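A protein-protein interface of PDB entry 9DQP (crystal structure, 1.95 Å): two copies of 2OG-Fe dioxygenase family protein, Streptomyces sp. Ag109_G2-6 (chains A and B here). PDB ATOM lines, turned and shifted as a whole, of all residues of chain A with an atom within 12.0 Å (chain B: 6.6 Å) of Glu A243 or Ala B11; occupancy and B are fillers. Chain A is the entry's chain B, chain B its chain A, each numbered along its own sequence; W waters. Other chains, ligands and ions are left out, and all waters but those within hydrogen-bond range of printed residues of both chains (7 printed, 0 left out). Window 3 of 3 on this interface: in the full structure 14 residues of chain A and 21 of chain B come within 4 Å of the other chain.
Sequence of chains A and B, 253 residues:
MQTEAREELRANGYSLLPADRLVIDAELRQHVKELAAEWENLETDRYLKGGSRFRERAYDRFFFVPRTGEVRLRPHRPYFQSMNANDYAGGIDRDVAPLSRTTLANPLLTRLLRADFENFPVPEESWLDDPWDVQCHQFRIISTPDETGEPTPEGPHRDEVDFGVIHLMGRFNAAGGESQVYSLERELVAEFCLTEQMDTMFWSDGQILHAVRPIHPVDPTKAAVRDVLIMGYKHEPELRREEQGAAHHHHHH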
ATOM      1  N   ARG A  61      31.632 -21.677 -14.436  1.00  0.00           N
ATOM      2  CA  ARG A  61      30.321 -21.810 -13.825  1.00  0.00           C
ATOM      3  C   ARG A  61      29.344 -22.309 -14.873  1.00  0.00           C
ATOM      4  O   ARG A  61      29.503 -22.031 -16.061  1.00  0.00           O
ATOM      5  CB  ARG A  61      29.806 -20.486 -13.273  1.00  0.00           C
ATOM      6  CG  ARG A  61      30.740 -19.792 -12.321  1.00  0.00           C
ATOM      7  CD  ARG A  61      30.161 -18.437 -11.944  1.00  0.00           C
ATOM      8  NE  ARG A  61      29.213 -18.539 -10.840  1.00  0.00           N
ATOM      9  CZ  ARG A  61      29.489 -18.212  -9.583  1.00  0.00           C
ATOM     10  NH1 ARG A  61      30.684 -17.759  -9.231  1.00  0.00           N
ATOM     11  NH2 ARG A  61      28.544 -18.333  -8.657  1.00  0.00           N
ATOM     12  N   PHE A  62      28.324 -23.036 -14.419  1.00  0.00           N
ATOM     13  CA  PHE A  62      27.304 -23.583 -15.299  1.00  0.00           C
ATOM     14  C   PHE A  62      25.928 -23.221 -14.781  1.00  0.00           C
ATOM     15  O   PHE A  62      25.702 -23.162 -13.572  1.00  0.00           O
ATOM     16  CB  PHE A  62      27.389 -25.119 -15.417  1.00  0.00           C
ATOM     17  CG  PHE A  62      28.683 -25.610 -15.968  1.00  0.00           C
ATOM     18  CD1 PHE A  62      29.750 -25.875 -15.125  1.00  0.00           C
ATOM     19  CD2 PHE A  62      28.830 -25.825 -17.321  1.00  0.00           C
ATOM     20  CE1 PHE A  62      30.952 -26.330 -15.637  1.00  0.00           C
ATOM     21  CE2 PHE A  62      30.024 -26.266 -17.841  1.00  0.00           C
ATOM     22  CZ  PHE A  62      31.088 -26.531 -16.999  1.00  0.00           C
ATOM     23  N   PHE A  63      25.033 -22.958 -15.723  1.00  0.00           N
ATOM     24  CA  PHE A  63      23.597 -22.950 -15.514  1.00  0.00           C
ATOM     25  C   PHE A  63      23.118 -24.400 -15.569  1.00  0.00           C
ATOM     26  O   PHE A  63      23.423 -25.110 -16.530  1.00  0.00           O
ATOM     27  CB  PHE A  63      22.966 -22.110 -16.631  1.00  0.00           C
ATOM     28  CG  PHE A  63      21.450 -22.071 -16.646  1.00  0.00           C
ATOM     29  CD1 PHE A  63      20.717 -23.077 -17.268  1.00  0.00           C
ATOM     30  CD2 PHE A  63      20.769 -20.967 -16.146  1.00  0.00           C
ATOM     31  CE1 PHE A  63      19.344 -23.018 -17.336  1.00  0.00           C
ATOM     32  CE2 PHE A  63      19.388 -20.891 -16.221  1.00  0.00           C
ATOM     33  CZ  PHE A  63      18.672 -21.921 -16.817  1.00  0.00           C
ATOM     34  N   GLU A  70      19.600 -29.854 -18.162  1.00  0.00           N
ATOM     35  CA  GLU A  70      20.189 -28.783 -18.949  1.00  0.00           C
ATOM     36  C   GLU A  70      21.421 -28.234 -18.234  1.00  0.00           C
ATOM     37  O   GLU A  70      21.380 -27.960 -17.035  1.00  0.00           O
ATOM     38  CB  GLU A  70      19.170 -27.675 -19.182  1.00  0.00           C
ATOM     39  CG  GLU A  70      19.705 -26.539 -20.046  1.00  0.00           C
ATOM     40  CD  GLU A  70      18.671 -25.443 -20.287  1.00  0.00           C
ATOM     41  OE1 GLU A  70      17.650 -25.414 -19.576  1.00  0.00           O
ATOM     42  OE2 GLU A  70      18.888 -24.614 -21.193  1.00  0.00           O
ATOM     43  N   VAL A  71      22.530 -28.136 -18.970  1.00  0.00           N
ATOM     44  CA  VAL A  71      23.797 -27.587 -18.489  1.00  0.00           C
ATOM     45  C   VAL A  71      24.289 -26.625 -19.560  1.00  0.00           C
ATOM     46  O   VAL A  71      24.402 -27.006 -20.729  1.00  0.00           O
ATOM     47  CB  VAL A  71      24.842 -28.693 -18.228  1.00  0.00           C
ATOM     48  CG1 VAL A  71      26.197 -28.098 -17.851  1.00  0.00           C
ATOM     49  CG2 VAL A  71      24.368 -29.622 -17.110  1.00  0.00           C
ATOM     50  N   ARG A  72      24.541 -25.372 -19.176  1.00  0.00           N
ATOM     51  CA  ARG A  72      25.049 -24.336 -20.067  1.00  0.00           C
ATOM     52  C   ARG A  72      26.263 -23.707 -19.403  1.00  0.00           C
ATOM     53  O   ARG A  72      26.167 -23.248 -18.267  1.00  0.00           O
ATOM     54  CB  ARG A  72      24.003 -23.234 -20.332  1.00  0.00           C
ATOM     55  CG  ARG A  72      22.669 -23.695 -20.912  1.00  0.00           C
ATOM     56  CD  ARG A  72      21.642 -22.553 -20.848  1.00  0.00           C
ATOM     57  NE  ARG A  72      22.155 -21.340 -21.473  1.00  0.00           N
ATOM     58  CZ  ARG A  72      22.003 -21.021 -22.749  1.00  0.00           C
ATOM     59  NH1 ARG A  72      21.355 -21.809 -23.591  1.00  0.00           N
ATOM     60  NH2 ARG A  72      22.508 -19.875 -23.193  1.00  0.00           N
ATOM     61  N   LEU A  73      27.394 -23.705 -20.097  1.00  0.00           N
ATOM     62  CA  LEU A  73      28.563 -22.995 -19.607  1.00  0.00           C
ATOM     63  C   LEU A  73      28.272 -21.501 -19.610  1.00  0.00           C
ATOM     64  O   LEU A  73      27.824 -20.955 -20.622  1.00  0.00           O
ATOM     65  CB  LEU A  73      29.768 -23.299 -20.497  1.00  0.00           C
ATOM     66  CG  LEU A  73      31.065 -22.527 -20.245  1.00  0.00           C
ATOM     67  CD1 LEU A  73      31.748 -23.016 -18.969  1.00  0.00           C
ATOM     68  CD2 LEU A  73      31.999 -22.619 -21.457  1.00  0.00           C
ATOM     69  N   ARG A  74      28.506 -20.844 -18.465  1.00  0.00           N
ATOM     70  CA  ARG A  74      28.238 -19.418 -18.344  1.00  0.00           C
ATOM     71  C   ARG A  74      29.469 -18.613 -18.743  1.00  0.00           C
ATOM     72  O   ARG A  74      30.592 -19.133 -18.743  1.00  0.00           O
ATOM     73  CB  ARG A  74      27.819 -19.091 -16.908  1.00  0.00           C
ATOM     74  CG  ARG A  74      26.524 -19.753 -16.476  1.00  0.00           C
ATOM     75  CD  ARG A  74      26.168 -19.454 -15.012  1.00  0.00           C
ATOM     76  NE  ARG A  74      25.908 -18.034 -14.822  1.00  0.00           N
ATOM     77  CZ  ARG A  74      25.728 -17.435 -13.653  1.00  0.00           C
ATOM     78  NH1 ARG A  74      25.759 -18.111 -12.522  1.00  0.00           N
ATOM     79  NH2 ARG A  74      25.529 -16.120 -13.623  1.00  0.00           N
ATOM     80  N   PRO A  75      29.292 -17.353 -19.156  1.00  0.00           N
ATOM     81  CA  PRO A  75      30.454 -16.531 -19.520  1.00  0.00           C
ATOM     82  C   PRO A  75      31.493 -16.576 -18.418  1.00  0.00           C
ATOM     83  O   PRO A  75      31.166 -16.507 -17.231  1.00  0.00           O
ATOM     84  CB  PRO A  75      29.869 -15.122 -19.672  1.00  0.00           C
ATOM     85  CG  PRO A  75      28.441 -15.323 -19.951  1.00  0.00           C
ATOM     86  CD  PRO A  75      28.027 -16.616 -19.299  1.00  0.00           C
ATOM     87  N   HIS A  76      32.751 -16.711 -18.817  1.00  0.00           N
ATOM     88  CA  HIS A  76      33.821 -16.854 -17.841  1.00  0.00           C
ATOM     89  C   HIS A  76      34.098 -15.513 -17.173  1.00  0.00           C
ATOM     90  O   HIS A  76      34.608 -14.588 -17.812  1.00  0.00           O
ATOM     91  CB  HIS A  76      35.086 -17.391 -18.500  1.00  0.00           C
ATOM     92  CG  HIS A  76      36.218 -17.555 -17.536  1.00  0.00           C
ATOM     93  ND1 HIS A  76      36.245 -18.553 -16.585  1.00  0.00           N
ATOM     94  CD2 HIS A  76      37.325 -16.804 -17.328  1.00  0.00           C
ATOM     95  CE1 HIS A  76      37.342 -18.433 -15.855  1.00  0.00           C
ATOM     96  NE2 HIS A  76      38.011 -17.378 -16.284  1.00  0.00           N
ATOM     97  N   ARG A  77      33.792 -15.405 -15.908  1.00  0.00           N
ATOM     98  CA  ARG A  77      34.119 -14.153 -15.236  1.00  0.00           C
ATOM     99  C   ARG A  77      35.534 -14.245 -14.671  1.00  0.00           C
ATOM    100  O   ARG A  77      35.859 -15.228 -13.992  1.00  0.00           O
ATOM    101  CB  ARG A  77      33.110 -13.851 -14.126  1.00  0.00           C
ATOM    102  CG  ARG A  77      31.686 -14.347 -14.392  1.00  0.00           C
ATOM    103  CD  ARG A  77      30.991 -13.594 -15.525  1.00  0.00           C
ATOM    104  NE  ARG A  77      29.614 -14.046 -15.714  1.00  0.00           N
ATOM    105  CZ  ARG A  77      28.553 -13.513 -15.119  1.00  0.00           C
ATOM    106  NH1 ARG A  77      28.665 -12.486 -14.286  1.00  0.00           N
ATOM    107  NH2 ARG A  77      27.346 -14.019 -15.368  1.00  0.00           N
ATOM    108  N   LEU A 239      17.998 -17.142 -11.756  1.00  0.00           N
ATOM    109  CA  LEU A 239      19.090 -17.146 -12.725  1.00  0.00           C
ATOM    110  C   LEU A 239      18.538 -17.302 -14.140  1.00  0.00           C
ATOM    111  O   LEU A 239      17.701 -18.168 -14.400  1.00  0.00           O
ATOM    112  CB  LEU A 239      20.074 -18.272 -12.414  1.00  0.00           C
ATOM    113  CG  LEU A 239      21.219 -18.443 -13.418  1.00  0.00           C
ATOM    114  CD1 LEU A 239      22.077 -17.188 -13.488  1.00  0.00           C
ATOM    115  CD2 LEU A 239      22.073 -19.672 -13.089  1.00  0.00           C
ATOM    116  N   ARG A 240      19.003 -16.473 -15.059  1.00  0.00           N
ATOM    117  CA  ARG A 240      18.519 -16.506 -16.427  1.00  0.00           C
ATOM    118  C   ARG A 240      19.610 -17.042 -17.340  1.00  0.00           C
ATOM    119  O   ARG A 240      20.798 -17.007 -17.001  1.00  0.00           O
ATOM    120  CB  ARG A 240      18.075 -15.111 -16.889  1.00  0.00           C
ATOM    121  CG  ARG A 240      16.820 -14.603 -16.195  1.00  0.00           C
ATOM    122  CD  ARG A 240      15.539 -14.974 -16.966  1.00  0.00           C
ATOM    123  NE  ARG A 240      15.313 -14.113 -18.124  1.00  0.00           N
ATOM    124  CZ  ARG A 240      15.514 -14.473 -19.388  1.00  0.00           C
ATOM    125  NH1 ARG A 240      15.900 -15.698 -19.709  1.00  0.00           N
ATOM    126  NH2 ARG A 240      15.323 -13.580 -20.354  1.00  0.00           N
ATOM    127  N   ARG A 241      19.198 -17.561 -18.494  1.00  0.00           N
ATOM    128  CA  ARG A 241      20.169 -18.037 -19.466  1.00  0.00           C
ATOM    129  C   ARG A 241      20.876 -16.858 -20.108  1.00  0.00           C
ATOM    130  O   ARG A 241      20.264 -15.824 -20.380  1.00  0.00           O
ATOM    131  CB  ARG A 241      19.502 -18.899 -20.540  1.00  0.00           C
ATOM    132  CG  ARG A 241      18.856 -20.142 -19.979  1.00  0.00           C
ATOM    133  CD  ARG A 241      18.227 -20.994 -21.088  1.00  0.00           C
ATOM    134  NE  ARG A 241      17.601 -22.162 -20.490  1.00  0.00           N
ATOM    135  CZ  ARG A 241      16.403 -22.147 -19.933  1.00  0.00           C
ATOM    136  NH1 ARG A 241      15.635 -21.070 -19.985  1.00  0.00           N
ATOM    137  NH2 ARG A 241      15.971 -23.230 -19.295  1.00  0.00           N
ATOM    138  N   GLU A 242      22.168 -17.033 -20.361  1.00  0.00           N
ATOM    139  CA  GLU A 242      23.044 -15.989 -20.874  1.00  0.00           C
ATOM    140  C   GLU A 242      23.517 -16.398 -22.261  1.00  0.00           C
ATOM    141  O   GLU A 242      23.959 -17.536 -22.457  1.00  0.00           O
ATOM    142  CB  GLU A 242      24.236 -15.771 -19.913  1.00  0.00           C
ATOM    143  CG  GLU A 242      23.796 -15.307 -18.507  1.00  0.00           C
ATOM    144  CD  GLU A 242      24.854 -15.515 -17.413  1.00  0.00           C
ATOM    145  OE1 GLU A 242      25.079 -16.671 -16.984  1.00  0.00           O
ATOM    146  OE2 GLU A 242      25.452 -14.511 -16.971  1.00  0.00           O
ATOM    147  N   GLU A 243      23.402 -15.488 -23.224  1.00  0.00           N
ATOM    148  CA  GLU A 243      23.896 -15.757 -24.569  1.00  0.00           C
ATOM    149  C   GLU A 243      24.971 -14.744 -24.970  1.00  0.00           C
ATOM    150  O   GLU A 243      26.169 -15.048 -24.949  1.00  0.00           O
ATOM    151  CB  GLU A 243      22.751 -15.745 -25.579  1.00  0.00           C
ATOM    152  CG  GLU A 243      23.040 -16.556 -26.835  1.00  0.00           C
ATOM    153  CD  GLU A 243      22.316 -17.893 -26.851  1.00  0.00           C
ATOM    154  OE1 GLU A 243      21.607 -18.209 -25.866  1.00  0.00           O
ATOM    155  OE2 GLU A 243      22.447 -18.628 -27.858  1.00  0.00           O
ATOM    156  N   ARG B   6       8.278 -20.183 -27.364  1.00  0.00           N
ATOM    157  CA  ARG B   6       8.605 -19.331 -28.504  1.00  0.00           C
ATOM    158  C   ARG B   6       9.725 -18.373 -28.154  1.00  0.00           C
ATOM    159  O   ARG B   6      10.625 -18.130 -28.963  1.00  0.00           O
ATOM    160  CB  ARG B   6       7.392 -18.519 -28.956  1.00  0.00           C
ATOM    161  CG  ARG B   6       6.256 -19.320 -29.503  1.00  0.00           C
ATOM    162  CD  ARG B   6       5.317 -18.390 -30.207  1.00  0.00           C
ATOM    163  NE  ARG B   6       4.062 -19.045 -30.519  1.00  0.00           N
ATOM    164  CZ  ARG B   6       3.350 -18.794 -31.607  1.00  0.00           C
ATOM    165  NH1 ARG B   6       3.784 -17.947 -32.534  1.00  0.00           N
ATOM    166  NH2 ARG B   6       2.183 -19.415 -31.774  1.00  0.00           N
ATOM    167  N   GLU B   7       9.677 -17.820 -26.952  1.00  0.00           N
ATOM    168  CA  GLU B   7      10.670 -16.831 -26.570  1.00  0.00           C
ATOM    169  C   GLU B   7      12.009 -17.496 -26.314  1.00  0.00           C
ATOM    170  O   GLU B   7      13.062 -16.946 -26.662  1.00  0.00           O
ATOM    171  CB  GLU B   7      10.190 -16.059 -25.342  1.00  0.00           C
ATOM    172  CG  GLU B   7      11.053 -14.844 -25.055  1.00  0.00           C
ATOM    173  CD  GLU B   7      11.388 -14.066 -26.322  1.00  0.00           C
ATOM    174  OE1 GLU B   7      10.452 -13.618 -27.033  1.00  0.00           O
ATOM    175  OE2 GLU B   7      12.598 -13.921 -26.618  1.00  0.00           O
ATOM    176  N   GLU B   8      11.981 -18.694 -25.724  1.00  0.00           N
ATOM    177  CA  GLU B   8      13.212 -19.454 -25.561  1.00  0.00           C
ATOM    178  C   GLU B   8      13.804 -19.825 -26.911  1.00  0.00           C
ATOM    179  O   GLU B   8      15.028 -19.727 -27.100  1.00  0.00           O
ATOM    180  CB  GLU B   8      12.951 -20.684 -24.684  1.00  0.00           C
ATOM    181  CG  GLU B   8      12.866 -20.318 -23.228  1.00  0.00           C
ATOM    182  CD  GLU B   8      12.407 -21.452 -22.340  1.00  0.00           C
ATOM    183  OE1 GLU B   8      12.278 -22.592 -22.825  1.00  0.00           O
ATOM    184  OE2 GLU B   8      12.161 -21.193 -21.144  1.00  0.00           O
ATOM    185  N   LEU B   9      12.965 -20.212 -27.884  1.00  0.00           N
ATOM    186  CA  LEU B   9      13.523 -20.496 -29.207  1.00  0.00           C
ATOM    187  C   LEU B   9      14.128 -19.238 -29.816  1.00  0.00           C
ATOM    188  O   LEU B   9      15.227 -19.276 -30.385  1.00  0.00           O
ATOM    189  CB  LEU B   9      12.464 -21.054 -30.156  1.00  0.00           C
ATOM    190  CG  LEU B   9      11.846 -22.457 -30.048  1.00  0.00           C
ATOM    191  CD1 LEU B   9      11.666 -23.115 -31.427  1.00  0.00           C
ATOM    192  CD2 LEU B   9      12.660 -23.303 -29.147  1.00  0.00           C
ATOM    193  N   ARG B  10      13.418 -18.115 -29.713  1.00  0.00           N
ATOM    194  CA  ARG B  10      13.963 -16.847 -30.197  1.00  0.00           C
ATOM    195  C   ARG B  10      15.313 -16.542 -29.550  1.00  0.00           C
ATOM    196  O   ARG B  10      16.305 -16.263 -30.238  1.00  0.00           O
ATOM    197  CB  ARG B  10      12.963 -15.719 -29.916  1.00  0.00           C
ATOM    198  CG  ARG B  10      12.427 -15.033 -31.165  1.00  0.00           C
ATOM    199  CD  ARG B  10      11.357 -13.992 -30.833  1.00  0.00           C
ATOM    200  NE  ARG B  10      10.051 -14.357 -31.375  1.00  0.00           N
ATOM    201  CZ  ARG B  10       8.997 -14.702 -30.645  1.00  0.00           C
ATOM    202  NH1 ARG B  10       9.041 -14.714 -29.324  1.00  0.00           N
ATOM    203  NH2 ARG B  10       7.862 -15.029 -31.257  1.00  0.00           N
ATOM    204  N   ALA B  11      15.373 -16.619 -28.224  1.00  0.00           N
ATOM    205  CA  ALA B  11      16.571 -16.186 -27.508  1.00  0.00           C
ATOM    206  C   ALA B  11      17.709 -17.197 -27.618  1.00  0.00           C
ATOM    207  O   ALA B  11      18.860 -16.819 -27.890  1.00  0.00           O
ATOM    208  CB  ALA B  11      16.231 -15.931 -26.039  1.00  0.00           C
ATOM    209  N   ASN B  12      17.419 -18.485 -27.388  1.00  0.00           N
ATOM    210  CA  ASN B  12      18.467 -19.499 -27.268  1.00  0.00           C
ATOM    211  C   ASN B  12      18.472 -20.533 -28.380  1.00  0.00           C
ATOM    212  O   ASN B  12      19.418 -21.318 -28.456  1.00  0.00           O
ATOM    213  CB  ASN B  12      18.346 -20.252 -25.944  1.00  0.00           C
ATOM    214  CG  ASN B  12      17.998 -19.360 -24.799  1.00  0.00           C
ATOM    215  OD1 ASN B  12      17.026 -19.605 -24.102  1.00  0.00           O
ATOM    216  ND2 ASN B  12      18.798 -18.316 -24.582  1.00  0.00           N
ATOM    217  N   GLY B  13      17.463 -20.556 -29.241  1.00  0.00           N
ATOM    218  CA  GLY B  13      17.423 -21.525 -30.315  1.00  0.00           C
ATOM    219  C   GLY B  13      16.833 -22.875 -29.937  1.00  0.00           C
ATOM    220  O   GLY B  13      16.701 -23.732 -30.816  1.00  0.00           O
ATOM    221  N   TYR B  14      16.471 -23.091 -28.670  1.00  0.00           N
ATOM    222  CA  TYR B  14      15.885 -24.367 -28.253  1.00  0.00           C
ATOM    223  C   TYR B  14      15.103 -24.141 -26.970  1.00  0.00           C
ATOM    224  O   TYR B  14      15.284 -23.134 -26.286  1.00  0.00           O
ATOM    225  CB  TYR B  14      16.961 -25.451 -28.047  1.00  0.00           C
ATOM    226  CG  TYR B  14      17.777 -25.194 -26.806  1.00  0.00           C
ATOM    227  CD1 TYR B  14      18.807 -24.266 -26.819  1.00  0.00           C
ATOM    228  CD2 TYR B  14      17.498 -25.860 -25.611  1.00  0.00           C
ATOM    229  CE1 TYR B  14      19.548 -24.005 -25.686  1.00  0.00           C
ATOM    230  CE2 TYR B  14      18.249 -25.603 -24.458  1.00  0.00           C
ATOM    231  CZ  TYR B  14      19.260 -24.664 -24.509  1.00  0.00           C
ATOM    232  OH  TYR B  14      19.996 -24.378 -23.373  1.00  0.00           O
ATOM    233  N   VAL B 189      26.969 -24.765 -26.587  1.00  0.00           N
ATOM    234  CA  VAL B 189      26.344 -23.820 -25.662  1.00  0.00           C
ATOM    235  C   VAL B 189      25.455 -24.492 -24.651  1.00  0.00           C
ATOM    236  O   VAL B 189      25.141 -23.850 -23.633  1.00  0.00           O
ATOM    237  CB  VAL B 189      25.540 -22.695 -26.350  1.00  0.00           C
ATOM    238  CG1 VAL B 189      26.451 -21.514 -26.779  1.00  0.00           C
ATOM    239  CG2 VAL B 189      24.637 -23.218 -27.419  1.00  0.00           C
ATOM    240  N   GLN B 207      19.079 -21.690 -36.517  1.00  0.00           N
ATOM    241  CA  GLN B 207      19.686 -20.842 -35.511  1.00  0.00           C
ATOM    242  C   GLN B 207      20.736 -21.552 -34.676  1.00  0.00           C
ATOM    243  O   GLN B 207      21.617 -20.885 -34.127  1.00  0.00           O
ATOM    244  CB  GLN B 207      18.597 -20.282 -34.598  1.00  0.00           C
ATOM    245  CG  GLN B 207      19.000 -19.188 -33.645  1.00  0.00           C
ATOM    246  CD  GLN B 207      17.794 -18.639 -32.912  1.00  0.00           C
ATOM    247  OE1 GLN B 207      16.717 -18.533 -33.486  1.00  0.00           O
ATOM    248  NE2 GLN B 207      17.957 -18.327 -31.629  1.00  0.00           N
ATOM    249  N   ILE B 208      20.671 -22.884 -34.565  1.00  0.00           N
ATOM    250  CA  ILE B 208      21.651 -23.666 -33.817  1.00  0.00           C
ATOM    251  C   ILE B 208      22.048 -24.854 -34.671  1.00  0.00           C
ATOM    252  O   ILE B 208      21.450 -25.132 -35.708  1.00  0.00           O
ATOM    253  CB  ILE B 208      21.111 -24.168 -32.459  1.00  0.00           C
ATOM    254  CG1 ILE B 208      19.821 -24.977 -32.674  1.00  0.00           C
ATOM    255  CG2 ILE B 208      20.871 -23.043 -31.523  1.00  0.00           C
ATOM    256  CD1 ILE B 208      19.403 -25.834 -31.448  1.00  0.00           C
HETATM  257  O   HOH W   1      21.734 -21.251 -26.499  1.00  0.00           O
HETATM  258  O   HOH W   2      18.700 -15.941 -22.767  1.00  0.00           O
HETATM  259  O   HOH W   3      15.670 -17.731 -22.104  1.00  0.00           O
HETATM  260  O   HOH W   4      16.445 -22.095 -23.784  1.00  0.00           O
HETATM  261  O   HOH W   5      27.168 -21.851 -23.387  1.00  0.00           O
HETATM  262  O   HOH W   6      13.082 -22.227 -18.724  1.00  0.00           O
HETATM  263  O   HOH W   7      27.954 -25.340 -22.568  1.00  0.00           O
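The side-chain hydroxyl (OH) of Tyr B14 is in hydrogen-bond range of the side-chain carboxylate (OE2) of Glu A70 (2.5 Å).
The side-chain hydroxyl (OH) of Tyr B14 lies within hydrogen-bond range of the guanidinium group (NH1) of Arg A72.
The side-chain carboxylate of Glu B8 lies within salt-bridge range of the guanidinium group of Arg A241, 3.7 Å away.
The side-chain carboxylate (OE1) of Glu A243 lies within hydrogen-bond range of the side-chain amide nitrogen (ND2) of Asn B12 (3.1 Å).
NH2 of Arg A72 is in salt-bridge range of OE1 of Glu A243 (3.3 Å).
The guanidinium group (NH2) of Arg A72 lies within hydrogen-bond range of the backbone carbonyl oxygen (O) of Glu A242, at 2.8 Å.
The backbone carbonyl oxygen (O) of Arg A72 is in hydrogen-bond range of the backbone NH (N) of Phe A63 (2.8 Å).
The backbone NH (N) of Gly B13 is in hydrogen-bond range of the backbone carbonyl oxygen (O) of Glu B8 (3.3 Å).
The side-chain carboxylate of Glu A70 is in salt-bridge range of the guanidinium group of Arg A241 (2.8 Å).
Among the printed residues, pairs that only touch across the chains: Arg A72 with Val B189 (3.5 Å), Arg A241 with Asn B12 (3.5 Å) and Glu A243 with Ala B11 (3.7 Å).
Printed residues of chain B within 4 Å of Glu A243: Ala B11 and Asn B12.
Of chain A, only Glu A243 comes within 4 Å of Ala B11.
No residue of chain A comes within 4 Å of Glu B7.
Of chain A, only Arg A72 (3.5 Å) comes within 4 Å of Val B189.
Of the printed residues of chain B, Glu A70 touches Tyr B14 (2.5 Å).
Of the printed residues of chain B, Arg A72 touches Tyr B14 (2.9 Å) and Val B189 (3.5 Å).
Printed residues of chain A within 4 Å of Glu B8: Arg A241 (3.7 Å).
Printed residues of chain B within 4 Å of Arg A241: Glu B8 and Asn B12.
Of the printed residues of chain A, Tyr B14 touches Glu A70 and Arg A72.
Arg A240 touches none of the printed residues of chain B.
Hydrophobic or aromatic side chains of chain B that line the printed part of chain A: Tyr B14.
Among the printed residues, Asp or Glu carboxylates within 4 Å of a Lys or Arg side-chain nitrogen of the other chain: Arg A241 with Glu B8 (3.7 Å).
No position is printed for both chains.
Water W6 lies within hydrogen-bond range of OE2 of Glu B8 (2.8 Å) and NH1 of Arg A241 (3.1 Å).
Water W2 lies within hydrogen-bond range of the backbone carbonyl oxygen (O) of Arg A241 and the side-chain amide nitrogen (ND2) of Asn B12.
Water W5 bridges the backbone carbonyl oxygen of Val B189 (2.9 Å) and the backbone carbonyl oxygen of Leu A73 (3.0 Å).
Water W1 lies within hydrogen-bond range of NH1 of Arg A72 (3.0 Å), O of Asn B12 (3.0 Å) and OE2 of Glu A243 (3.0 Å).
Water W7 bridges the backbone NH of Leu A73 and the backbone carbonyl oxygen of Val B189.
Water W3 bridges the side-chain amide oxygen of Asn B12 (3.1 Å) and the guanidinium group of Arg A240 (3.1 Å).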
